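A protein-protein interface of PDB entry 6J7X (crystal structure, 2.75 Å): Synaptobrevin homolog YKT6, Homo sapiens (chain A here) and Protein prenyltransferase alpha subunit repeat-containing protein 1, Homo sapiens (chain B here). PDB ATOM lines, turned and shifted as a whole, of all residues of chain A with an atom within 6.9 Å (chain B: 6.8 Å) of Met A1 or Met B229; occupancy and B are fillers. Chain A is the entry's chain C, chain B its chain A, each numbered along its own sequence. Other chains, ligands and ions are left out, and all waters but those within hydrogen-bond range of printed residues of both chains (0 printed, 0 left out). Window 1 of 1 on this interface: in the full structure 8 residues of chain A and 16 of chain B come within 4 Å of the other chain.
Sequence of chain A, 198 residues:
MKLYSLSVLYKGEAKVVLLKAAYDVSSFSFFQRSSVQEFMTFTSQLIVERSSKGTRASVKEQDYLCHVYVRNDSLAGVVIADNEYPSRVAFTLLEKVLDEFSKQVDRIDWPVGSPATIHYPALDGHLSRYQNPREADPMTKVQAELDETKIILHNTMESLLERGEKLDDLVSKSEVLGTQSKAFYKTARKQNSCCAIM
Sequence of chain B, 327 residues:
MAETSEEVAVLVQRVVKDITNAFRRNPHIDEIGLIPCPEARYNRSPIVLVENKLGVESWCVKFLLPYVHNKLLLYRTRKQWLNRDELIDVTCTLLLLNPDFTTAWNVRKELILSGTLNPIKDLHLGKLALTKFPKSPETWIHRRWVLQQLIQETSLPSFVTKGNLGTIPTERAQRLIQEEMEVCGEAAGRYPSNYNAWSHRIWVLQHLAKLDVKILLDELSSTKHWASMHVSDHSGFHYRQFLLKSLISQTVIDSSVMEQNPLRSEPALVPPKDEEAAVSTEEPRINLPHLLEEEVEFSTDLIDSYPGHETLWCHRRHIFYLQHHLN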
ATOM      1  N   MET A   1     -27.097  -3.056  18.424  1.00  0.00           N
ATOM      2  CA  MET A   1     -26.332  -2.539  17.295  1.00  0.00           C
ATOM      3  C   MET A   1     -25.592  -3.657  16.570  1.00  0.00           C
ATOM      4  O   MET A   1     -24.417  -3.903  16.838  1.00  0.00           O
ATOM      5  CB  MET A   1     -25.331  -1.478  17.763  1.00  0.00           C
ATOM      6  CG  MET A   1     -25.942  -0.300  18.509  1.00  0.00           C
ATOM      7  SD  MET A   1     -27.092   0.662  17.510  1.00  0.00           S
ATOM      8  CE  MET A   1     -26.165   0.820  15.993  1.00  0.00           C
ATOM      9  N   LYS A   2     -26.279  -4.331  15.652  1.00  0.00           N
ATOM     10  CA  LYS A   2     -25.674  -5.439  14.918  1.00  0.00           C
ATOM     11  C   LYS A   2     -26.132  -5.493  13.463  1.00  0.00           C
ATOM     12  O   LYS A   2     -27.261  -5.131  13.143  1.00  0.00           O
ATOM     13  CB  LYS A   2     -25.990  -6.772  15.605  1.00  0.00           C
ATOM     14  CG  LYS A   2     -25.205  -7.027  16.885  1.00  0.00           C
ATOM     15  CD  LYS A   2     -25.508  -8.400  17.462  1.00  0.00           C
ATOM     16  CE  LYS A   2     -26.928  -8.479  17.999  1.00  0.00           C
ATOM     17  NZ  LYS A   2     -27.135  -7.568  19.158  1.00  0.00           N
ATOM     18  N   LEU A   3     -25.239  -5.946  12.588  1.00  0.00           N
ATOM     19  CA  LEU A   3     -25.573  -6.192  11.188  1.00  0.00           C
ATOM     20  C   LEU A   3     -25.517  -7.687  10.899  1.00  0.00           C
ATOM     21  O   LEU A   3     -24.555  -8.360  11.266  1.00  0.00           O
ATOM     22  CB  LEU A   3     -24.624  -5.437  10.256  1.00  0.00           C
ATOM     23  CG  LEU A   3     -24.747  -3.914  10.192  1.00  0.00           C
ATOM     24  CD1 LEU A   3     -23.723  -3.341   9.227  1.00  0.00           C
ATOM     25  CD2 LEU A   3     -26.154  -3.504   9.785  1.00  0.00           C
ATOM     26  N   ALA A  81     -30.608  -5.990   9.868  1.00  0.00           N
ATOM     27  CA  ALA A  81     -30.075  -5.592  11.165  1.00  0.00           C
ATOM     28  C   ALA A  81     -31.137  -5.709  12.255  1.00  0.00           C
ATOM     29  O   ALA A  81     -32.226  -6.231  12.020  1.00  0.00           O
ATOM     30  CB  ALA A  81     -29.536  -4.172  11.100  1.00  0.00           C
ATOM     31  N   ASP A  82     -30.813  -5.218  13.447  1.00  0.00           N
ATOM     32  CA  ASP A  82     -31.763  -5.209  14.553  1.00  0.00           C
ATOM     33  C   ASP A  82     -32.519  -3.884  14.609  1.00  0.00           C
ATOM     34  O   ASP A  82     -32.384  -3.044  13.720  1.00  0.00           O
ATOM     35  CB  ASP A  82     -31.051  -5.471  15.883  1.00  0.00           C
ATOM     36  CG  ASP A  82     -29.848  -4.569  16.097  1.00  0.00           C
ATOM     37  OD1 ASP A  82     -29.679  -3.597  15.331  1.00  0.00           O
ATOM     38  OD2 ASP A  82     -29.071  -4.831  17.039  1.00  0.00           O
ATOM     39  N   ASN A  83     -33.311  -3.705  15.661  1.00  0.00           N
ATOM     40  CA  ASN A  83     -34.095  -2.487  15.829  1.00  0.00           C
ATOM     41  C   ASN A  83     -33.225  -1.292  16.204  1.00  0.00           C
ATOM     42  O   ASN A  83     -33.563  -0.148  15.901  1.00  0.00           O
ATOM     43  CB  ASN A  83     -35.176  -2.693  16.892  1.00  0.00           C
ATOM     44  CG  ASN A  83     -36.146  -3.801  16.529  1.00  0.00           C
ATOM     45  OD1 ASN A  83     -36.469  -4.003  15.358  1.00  0.00           O
ATOM     46  ND2 ASN A  83     -36.614  -4.529  17.536  1.00  0.00           N
ATOM     47  N   GLU A  84     -32.102  -1.566  16.862  1.00  0.00           N
ATOM     48  CA  GLU A  84     -31.217  -0.511  17.341  1.00  0.00           C
ATOM     49  C   GLU A  84     -30.496   0.211  16.210  1.00  0.00           C
ATOM     50  O   GLU A  84     -30.311   1.428  16.262  1.00  0.00           O
ATOM     51  CB  GLU A  84     -30.186  -1.083  18.316  1.00  0.00           C
ATOM     52  CG  GLU A  84     -30.760  -1.520  19.652  1.00  0.00           C
ATOM     53  CD  GLU A  84     -29.681  -1.784  20.682  1.00  0.00           C
ATOM     54  OE1 GLU A  84     -30.022  -1.980  21.867  1.00  0.00           O
ATOM     55  OE2 GLU A  84     -28.489  -1.791  20.306  1.00  0.00           O
ATOM     56  N   TYR A  85     -30.082  -0.541  15.194  1.00  0.00           N
ATOM     57  CA  TYR A  85     -29.317   0.030  14.090  1.00  0.00           C
ATOM     58  C   TYR A  85     -30.154   1.042  13.315  1.00  0.00           C
ATOM     59  O   TYR A  85     -31.196   0.695  12.757  1.00  0.00           O
ATOM     60  CB  TYR A  85     -28.817  -1.072  13.153  1.00  0.00           C
ATOM     61  CG  TYR A  85     -27.527  -0.719  12.448  1.00  0.00           C
ATOM     62  CD1 TYR A  85     -27.535   0.004  11.261  1.00  0.00           C
ATOM     63  CD2 TYR A  85     -26.301  -1.105  12.971  1.00  0.00           C
ATOM     64  CE1 TYR A  85     -26.356   0.330  10.617  1.00  0.00           C
ATOM     65  CE2 TYR A  85     -25.117  -0.785  12.334  1.00  0.00           C
ATOM     66  CZ  TYR A  85     -25.151  -0.068  11.158  1.00  0.00           C
ATOM     67  OH  TYR A  85     -23.974   0.253  10.521  1.00  0.00           O
ATOM     68  N   PRO A  86     -29.694   2.304  13.283  1.00  0.00           N
ATOM     69  CA  PRO A  86     -30.404   3.407  12.626  1.00  0.00           C
ATOM     70  C   PRO A  86     -30.592   3.168  11.132  1.00  0.00           C
ATOM     71  O   PRO A  86     -29.682   2.683  10.462  1.00  0.00           O
ATOM     72  CB  PRO A  86     -29.493   4.614  12.879  1.00  0.00           C
ATOM     73  CG  PRO A  86     -28.150   4.030  13.148  1.00  0.00           C
ATOM     74  CD  PRO A  86     -28.409   2.740  13.855  1.00  0.00           C
ATOM     75  N   TYR A 130     -19.006  -1.642   9.270  1.00  0.00           N
ATOM     76  CA  TYR A 130     -20.190  -0.870   9.629  1.00  0.00           C
ATOM     77  C   TYR A 130     -20.975  -1.491  10.781  1.00  0.00           C
ATOM     78  O   TYR A 130     -22.134  -1.142  11.007  1.00  0.00           O
ATOM     79  CB  TYR A 130     -21.101  -0.709   8.411  1.00  0.00           C
ATOM     80  CG  TYR A 130     -20.735   0.461   7.529  1.00  0.00           C
ATOM     81  CD1 TYR A 130     -19.588   0.436   6.746  1.00  0.00           C
ATOM     82  CD2 TYR A 130     -21.540   1.592   7.475  1.00  0.00           C
ATOM     83  CE1 TYR A 130     -19.251   1.507   5.939  1.00  0.00           C
ATOM     84  CE2 TYR A 130     -21.212   2.665   6.671  1.00  0.00           C
ATOM     85  CZ  TYR A 130     -20.068   2.617   5.905  1.00  0.00           C
ATOM     86  OH  TYR A 130     -19.740   3.687   5.104  1.00  0.00           O
ATOM     87  N   GLN A 131     -20.343  -2.405  11.509  1.00  0.00           N
ATOM     88  CA  GLN A 131     -20.973  -3.023  12.670  1.00  0.00           C
ATOM     89  C   GLN A 131     -21.225  -1.968  13.741  1.00  0.00           C
ATOM     90  O   GLN A 131     -22.209  -2.032  14.476  1.00  0.00           O
ATOM     91  CB  GLN A 131     -20.102  -4.154  13.222  1.00  0.00           C
ATOM     92  CG  GLN A 131     -20.868  -5.194  14.023  1.00  0.00           C
ATOM     93  CD  GLN A 131     -21.793  -6.031  13.157  1.00  0.00           C
ATOM     94  OE1 GLN A 131     -22.848  -6.474  13.606  1.00  0.00           O
ATOM     95  NE2 GLN A 131     -21.394  -6.255  11.909  1.00  0.00           N
ATOM     96  N   ASN A 132     -20.324  -0.994  13.815  1.00  0.00           N
ATOM     97  CA  ASN A 132     -20.479   0.142  14.714  1.00  0.00           C
ATOM     98  C   ASN A 132     -20.514   1.444  13.919  1.00  0.00           C
ATOM     99  O   ASN A 132     -19.498   1.860  13.363  1.00  0.00           O
ATOM    100  CB  ASN A 132     -19.343   0.175  15.739  1.00  0.00           C
ATOM    101  CG  ASN A 132     -19.647   1.080  16.917  1.00  0.00           C
ATOM    102  OD1 ASN A 132     -20.632   1.818  16.911  1.00  0.00           O
ATOM    103  ND2 ASN A 132     -18.794   1.032  17.934  1.00  0.00           N
ATOM    104  N   PRO A 133     -21.690   2.088  13.859  1.00  0.00           N
ATOM    105  CA  PRO A 133     -21.907   3.324  13.093  1.00  0.00           C
ATOM    106  C   PRO A 133     -20.988   4.472  13.506  1.00  0.00           C
ATOM    107  O   PRO A 133     -20.770   5.391  12.716  1.00  0.00           O
ATOM    108  CB  PRO A 133     -23.366   3.670  13.397  1.00  0.00           C
ATOM    109  CG  PRO A 133     -23.992   2.369  13.721  1.00  0.00           C
ATOM    110  CD  PRO A 133     -22.940   1.600  14.464  1.00  0.00           C
ATOM    111  N   ARG A 134     -20.459   4.419  14.724  1.00  0.00           N
ATOM    112  CA  ARG A 134     -19.529   5.439  15.193  1.00  0.00           C
ATOM    113  C   ARG A 134     -18.161   5.242  14.549  1.00  0.00           C
ATOM    114  O   ARG A 134     -17.293   6.113  14.622  1.00  0.00           O
ATOM    115  CB  ARG A 134     -19.411   5.405  16.718  1.00  0.00           C
ATOM    116  CG  ARG A 134     -20.690   4.987  17.422  1.00  0.00           C
ATOM    117  CD  ARG A 134     -20.790   5.593  18.810  1.00  0.00           C
ATOM    118  NE  ARG A 134     -21.142   7.009  18.750  1.00  0.00           N
ATOM    119  CZ  ARG A 134     -21.331   7.778  19.817  1.00  0.00           C
ATOM    120  NH1 ARG A 134     -21.197   7.270  21.034  1.00  0.00           N
ATOM    121  NH2 ARG A 134     -21.650   9.056  19.666  1.00  0.00           N
ATOM    122  N   GLU A 135     -17.980   4.087  13.915  1.00  0.00           N
ATOM    123  CA  GLU A 135     -16.741   3.767  13.220  1.00  0.00           C
ATOM    124  C   GLU A 135     -16.973   3.706  11.714  1.00  0.00           C
ATOM    125  O   GLU A 135     -16.257   3.014  10.990  1.00  0.00           O
ATOM    126  CB  GLU A 135     -16.173   2.439  13.726  1.00  0.00           C
ATOM    127  CG  GLU A 135     -15.907   2.415  15.224  1.00  0.00           C
ATOM    128  CD  GLU A 135     -15.652   1.016  15.751  1.00  0.00           C
ATOM    129  OE1 GLU A 135     -15.801   0.049  14.974  1.00  0.00           O
ATOM    130  OE2 GLU A 135     -15.307   0.882  16.944  1.00  0.00           O
ATOM    131  N   LYS B 224     -18.420  -0.150  29.114  1.00  0.00           N
ATOM    132  CA  LYS B 224     -18.681   1.061  28.341  1.00  0.00           C
ATOM    133  C   LYS B 224     -18.940   0.740  26.873  1.00  0.00           C
ATOM    134  O   LYS B 224     -19.923   1.201  26.293  1.00  0.00           O
ATOM    135  CB  LYS B 224     -17.515   2.047  28.455  1.00  0.00           C
ATOM    136  CG  LYS B 224     -17.484   2.828  29.757  1.00  0.00           C
ATOM    137  CD  LYS B 224     -16.423   3.918  29.729  1.00  0.00           C
ATOM    138  CE  LYS B 224     -16.760   4.994  28.710  1.00  0.00           C
ATOM    139  NZ  LYS B 224     -18.030   5.697  29.043  1.00  0.00           N
ATOM    140  N   HIS B 225     -18.054  -0.053  26.280  1.00  0.00           N
ATOM    141  CA  HIS B 225     -18.185  -0.423  24.878  1.00  0.00           C
ATOM    142  C   HIS B 225     -19.429  -1.273  24.646  1.00  0.00           C
ATOM    143  O   HIS B 225     -20.123  -1.111  23.641  1.00  0.00           O
ATOM    144  CB  HIS B 225     -16.942  -1.175  24.400  1.00  0.00           C
ATOM    145  CG  HIS B 225     -16.985  -1.550  22.951  1.00  0.00           C
ATOM    146  ND1 HIS B 225     -17.317  -2.816  22.520  1.00  0.00           N
ATOM    147  CD2 HIS B 225     -16.746  -0.823  21.834  1.00  0.00           C
ATOM    148  CE1 HIS B 225     -17.276  -2.855  21.200  1.00  0.00           C
ATOM    149  NE2 HIS B 225     -16.933  -1.658  20.759  1.00  0.00           N
ATOM    150  N   TRP B 226     -19.708  -2.174  25.582  1.00  0.00           N
ATOM    151  CA  TRP B 226     -20.864  -3.055  25.475  1.00  0.00           C
ATOM    152  C   TRP B 226     -22.166  -2.263  25.542  1.00  0.00           C
ATOM    153  O   TRP B 226     -23.091  -2.507  24.766  1.00  0.00           O
ATOM    154  CB  TRP B 226     -20.838  -4.116  26.579  1.00  0.00           C
ATOM    155  CG  TRP B 226     -21.796  -5.247  26.348  1.00  0.00           C
ATOM    156  CD1 TRP B 226     -21.512  -6.459  25.789  1.00  0.00           C
ATOM    157  CD2 TRP B 226     -23.195  -5.270  26.663  1.00  0.00           C
ATOM    158  NE1 TRP B 226     -22.645  -7.235  25.740  1.00  0.00           N
ATOM    159  CE2 TRP B 226     -23.691  -6.528  26.271  1.00  0.00           C
ATOM    160  CE3 TRP B 226     -24.075  -4.350  27.242  1.00  0.00           C
ATOM    161  CZ2 TRP B 226     -25.026  -6.889  26.436  1.00  0.00           C
ATOM    162  CZ3 TRP B 226     -25.400  -4.710  27.405  1.00  0.00           C
ATOM    163  CH2 TRP B 226     -25.862  -5.968  27.004  1.00  0.00           C
ATOM    164  N   ALA B 227     -22.229  -1.314  26.471  1.00  0.00           N
ATOM    165  CA  ALA B 227     -23.432  -0.514  26.677  1.00  0.00           C
ATOM    166  C   ALA B 227     -23.746   0.359  25.467  1.00  0.00           C
ATOM    167  O   ALA B 227     -24.910   0.648  25.188  1.00  0.00           O
ATOM    168  CB  ALA B 227     -23.286   0.346  27.924  1.00  0.00           C
ATOM    169  N   SER B 228     -22.707   0.776  24.752  1.00  0.00           N
ATOM    170  CA  SER B 228     -22.880   1.613  23.569  1.00  0.00           C
ATOM    171  C   SER B 228     -23.355   0.792  22.375  1.00  0.00           C
ATOM    172  O   SER B 228     -23.831   1.343  21.381  1.00  0.00           O
ATOM    173  CB  SER B 228     -21.576   2.336  23.225  1.00  0.00           C
ATOM    174  OG  SER B 228     -20.551   1.414  22.898  1.00  0.00           O
ATOM    175  N   MET B 229     -23.219  -0.527  22.477  1.00  0.00           N
ATOM    176  CA  MET B 229     -23.634  -1.428  21.407  1.00  0.00           C
ATOM    177  C   MET B 229     -24.956  -2.110  21.740  1.00  0.00           C
ATOM    178  O   MET B 229     -25.448  -2.944  20.979  1.00  0.00           O
ATOM    179  CB  MET B 229     -22.551  -2.473  21.138  1.00  0.00           C
ATOM    180  CG  MET B 229     -21.245  -1.885  20.626  1.00  0.00           C
ATOM    181  SD  MET B 229     -21.445  -1.030  19.050  1.00  0.00           S
ATOM    182  CE  MET B 229     -21.798  -2.405  17.961  1.00  0.00           C
ATOM    183  N   HIS B 230     -25.526  -1.749  22.886  1.00  0.00           N
ATOM    184  CA  HIS B 230     -26.832  -2.247  23.300  1.00  0.00           C
ATOM    185  C   HIS B 230     -27.616  -1.130  23.981  1.00  0.00           C
ATOM    186  O   HIS B 230     -27.799  -1.140  25.199  1.00  0.00           O
ATOM    187  CB  HIS B 230     -26.689  -3.449  24.239  1.00  0.00           C
ATOM    188  CG  HIS B 230     -25.985  -4.618  23.623  1.00  0.00           C
ATOM    189  ND1 HIS B 230     -24.624  -4.812  23.734  1.00  0.00           N
ATOM    190  CD2 HIS B 230     -26.454  -5.654  22.887  1.00  0.00           C
ATOM    191  CE1 HIS B 230     -24.286  -5.918  23.095  1.00  0.00           C
ATOM    192  NE2 HIS B 230     -25.377  -6.447  22.572  1.00  0.00           N
ATOM    193  N   VAL B 231     -28.079  -0.172  23.186  1.00  0.00           N
ATOM    194  CA  VAL B 231     -28.690   1.044  23.718  1.00  0.00           C
ATOM    195  C   VAL B 231     -30.124   0.843  24.206  1.00  0.00           C
ATOM    196  O   VAL B 231     -30.669   1.698  24.904  1.00  0.00           O
ATOM    197  CB  VAL B 231     -28.679   2.173  22.667  1.00  0.00           C
ATOM    198  CG1 VAL B 231     -27.250   2.568  22.330  1.00  0.00           C
ATOM    199  CG2 VAL B 231     -29.428   1.743  21.414  1.00  0.00           C
ATOM    200  N   SER B 232     -30.734  -0.281  23.843  1.00  0.00           N
ATOM    201  CA  SER B 232     -32.103  -0.565  24.263  1.00  0.00           C
ATOM    202  C   SER B 232     -32.131  -1.544  25.431  1.00  0.00           C
ATOM    203  O   SER B 232     -33.112  -2.262  25.628  1.00  0.00           O
ATOM    204  CB  SER B 232     -32.921  -1.120  23.095  1.00  0.00           C
ATOM    205  OG  SER B 232     -32.411  -2.368  22.662  1.00  0.00           O
ATOM    206  N   PHE B 237     -27.832  -0.869  31.499  1.00  0.00           N
ATOM    207  CA  PHE B 237     -27.588   0.500  31.932  1.00  0.00           C
ATOM    208  C   PHE B 237     -27.879   0.689  33.417  1.00  0.00           C
ATOM    209  O   PHE B 237     -27.300   1.566  34.057  1.00  0.00           O
ATOM    210  CB  PHE B 237     -28.416   1.480  31.101  1.00  0.00           C
ATOM    211  CG  PHE B 237     -27.820   1.777  29.756  1.00  0.00           C
ATOM    212  CD1 PHE B 237     -26.785   2.686  29.634  1.00  0.00           C
ATOM    213  CD2 PHE B 237     -28.284   1.139  28.619  1.00  0.00           C
ATOM    214  CE1 PHE B 237     -26.227   2.958  28.403  1.00  0.00           C
ATOM    215  CE2 PHE B 237     -27.730   1.409  27.383  1.00  0.00           C
ATOM    216  CZ  PHE B 237     -26.699   2.320  27.276  1.00  0.00           C
ATOM    217  N   PHE B 298     -21.530  10.604  28.196  1.00  0.00           N
ATOM    218  CA  PHE B 298     -21.606   9.346  27.463  1.00  0.00           C
ATOM    219  C   PHE B 298     -23.039   9.046  27.034  1.00  0.00           C
ATOM    220  O   PHE B 298     -23.276   8.547  25.933  1.00  0.00           O
ATOM    221  CB  PHE B 298     -21.055   8.201  28.318  1.00  0.00           C
ATOM    222  CG  PHE B 298     -21.213   6.842  27.697  1.00  0.00           C
ATOM    223  CD1 PHE B 298     -20.342   6.409  26.712  1.00  0.00           C
ATOM    224  CD2 PHE B 298     -22.225   5.991  28.111  1.00  0.00           C
ATOM    225  CE1 PHE B 298     -20.484   5.157  26.142  1.00  0.00           C
ATOM    226  CE2 PHE B 298     -22.372   4.738  27.546  1.00  0.00           C
ATOM    227  CZ  PHE B 298     -21.500   4.321  26.560  1.00  0.00           C
ATOM    228  N   LEU B 302     -24.890   9.321  23.106  1.00  0.00           N
ATOM    229  CA  LEU B 302     -25.626   8.207  22.516  1.00  0.00           C
ATOM    230  C   LEU B 302     -27.034   8.623  22.096  1.00  0.00           C
ATOM    231  O   LEU B 302     -27.526   8.195  21.053  1.00  0.00           O
ATOM    232  CB  LEU B 302     -25.699   7.035  23.495  1.00  0.00           C
ATOM    233  CG  LEU B 302     -24.391   6.284  23.750  1.00  0.00           C
ATOM    234  CD1 LEU B 302     -24.600   5.173  24.766  1.00  0.00           C
ATOM    235  CD2 LEU B 302     -23.836   5.727  22.449  1.00  0.00           C
ATOM    236  N   TYR B 306     -28.226   8.014  18.711  1.00  0.00           N
ATOM    237  CA  TYR B 306     -29.348   7.095  18.565  1.00  0.00           C
ATOM    238  C   TYR B 306     -30.576   7.592  19.321  1.00  0.00           C
ATOM    239  O   TYR B 306     -30.779   7.241  20.484  1.00  0.00           O
ATOM    240  CB  TYR B 306     -28.962   5.699  19.057  1.00  0.00           C
ATOM    241  CG  TYR B 306     -27.574   5.264  18.646  1.00  0.00           C
ATOM    242  CD1 TYR B 306     -27.303   4.875  17.341  1.00  0.00           C
ATOM    243  CD2 TYR B 306     -26.534   5.236  19.568  1.00  0.00           C
ATOM    244  CE1 TYR B 306     -26.035   4.473  16.963  1.00  0.00           C
ATOM    245  CE2 TYR B 306     -25.263   4.836  19.200  1.00  0.00           C
ATOM    246  CZ  TYR B 306     -25.020   4.456  17.897  1.00  0.00           C
ATOM    247  OH  TYR B 306     -23.757   4.055  17.527  1.00  0.00           O
ATOM    248  N   HIS B 309     -34.734   6.130  22.144  1.00  0.00           N
ATOM    249  CA  HIS B 309     -34.530   5.072  23.127  1.00  0.00           C
ATOM    250  C   HIS B 309     -34.809   5.572  24.540  1.00  0.00           C
ATOM    251  O   HIS B 309     -34.015   6.324  25.104  1.00  0.00           O
ATOM    252  CB  HIS B 309     -33.103   4.524  23.038  1.00  0.00           C
ATOM    253  CG  HIS B 309     -32.793   3.844  21.741  1.00  0.00           C
ATOM    254  ND1 HIS B 309     -33.185   2.551  21.466  1.00  0.00           N
ATOM    255  CD2 HIS B 309     -32.128   4.277  20.644  1.00  0.00           C
ATOM    256  CE1 HIS B 309     -32.775   2.217  20.255  1.00  0.00           C
ATOM    257  NE2 HIS B 309     -32.132   3.246  19.735  1.00  0.00           N
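OE2 of Glu A84 sits close to O of Met B229, at 3.3 Å. OG of Ser B232 lies within hydrogen-bond range of OE1 of Glu A84, 2.5 Å away. ND2 of Asn A132 lies close to SD of Met B229 (3.5 Å). N of Met A1 lies within hydrogen-bond range of O of Met B229 (3.0 Å). The backbone NH (N) of Val B231 is in hydrogen-bond range of the side-chain carboxylate (OE1) of Glu A84.
ND1 of His B230 is in hydrogen-bond range of O of Trp B226, at 3.0 Å. OD2 of Asp A82 lies within hydrogen-bond range of N of Met A1, at 3.0 Å. OG of Ser B228 is in hydrogen-bond range of O of Lys B224 (3.5 Å). The side-chain amide oxygen (OD1) of Asn A132 sits close to the backbone NH (N) of Arg A134 (3.4 Å). O of His B225 sits at hydrogen-bond distance from OG of Ser B228. The side-chain carboxylate of Glu A84 is in hydrogen-bond range of the backbone NH of Met A1 (2.7 Å).
O of Ser B228 touches CG of Met A1 (3.9 Å). Tyr B306 touches Met A1. Glu A84 touches His B230. Gln A131 touches Met B229. Asn A132 touches Tyr B306. Arg A134 touches Leu B302 (NH1 to CD2, 3.4 Å). CG of Arg A134 touches OH of Tyr B306 (3.2 Å).
Of chain B, only Ser B228 (3.9 Å), Met B229 (3.0 Å) and Tyr B306 (3.8 Å) come within 4 Å of Met A1. Lys A2 touches none of the printed residues of chain B. Of the printed residues of chain B, Arg A134 touches Leu B302 and Tyr B306. Met B229 touches just these residues of chain A: Met A1, Glu A84, Gln A131 and Asn A132. Of the printed residues of chain A, Val B231 touches Glu A84 (3.0 Å). Phe B298 touches none of the printed residues of chain A. The nearest residue of chain A that does not touch Met B229 is Lys A2 (5.2 Å). The nearest printed residue of chain A that does not touch Ser B228 is Asn A132 (5.3 Å).
Of the 14 printed residues of chain B, 7 touch a printed residue of chain A. Hydrophobic or aromatic side chains of chain B within 4 Å of the printed part of chain A: Met B229, Val B231, Leu B302 and Tyr B306. Of the 15 printed residues of chain A, 5 touch a printed residue of chain B. Among the printed residues, 12 pairs touch across the chains. Among the printed residues, no Asp or Glu carboxylate lies within 4 Å of a Lys or Arg side-chain nitrogen of the other chain.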
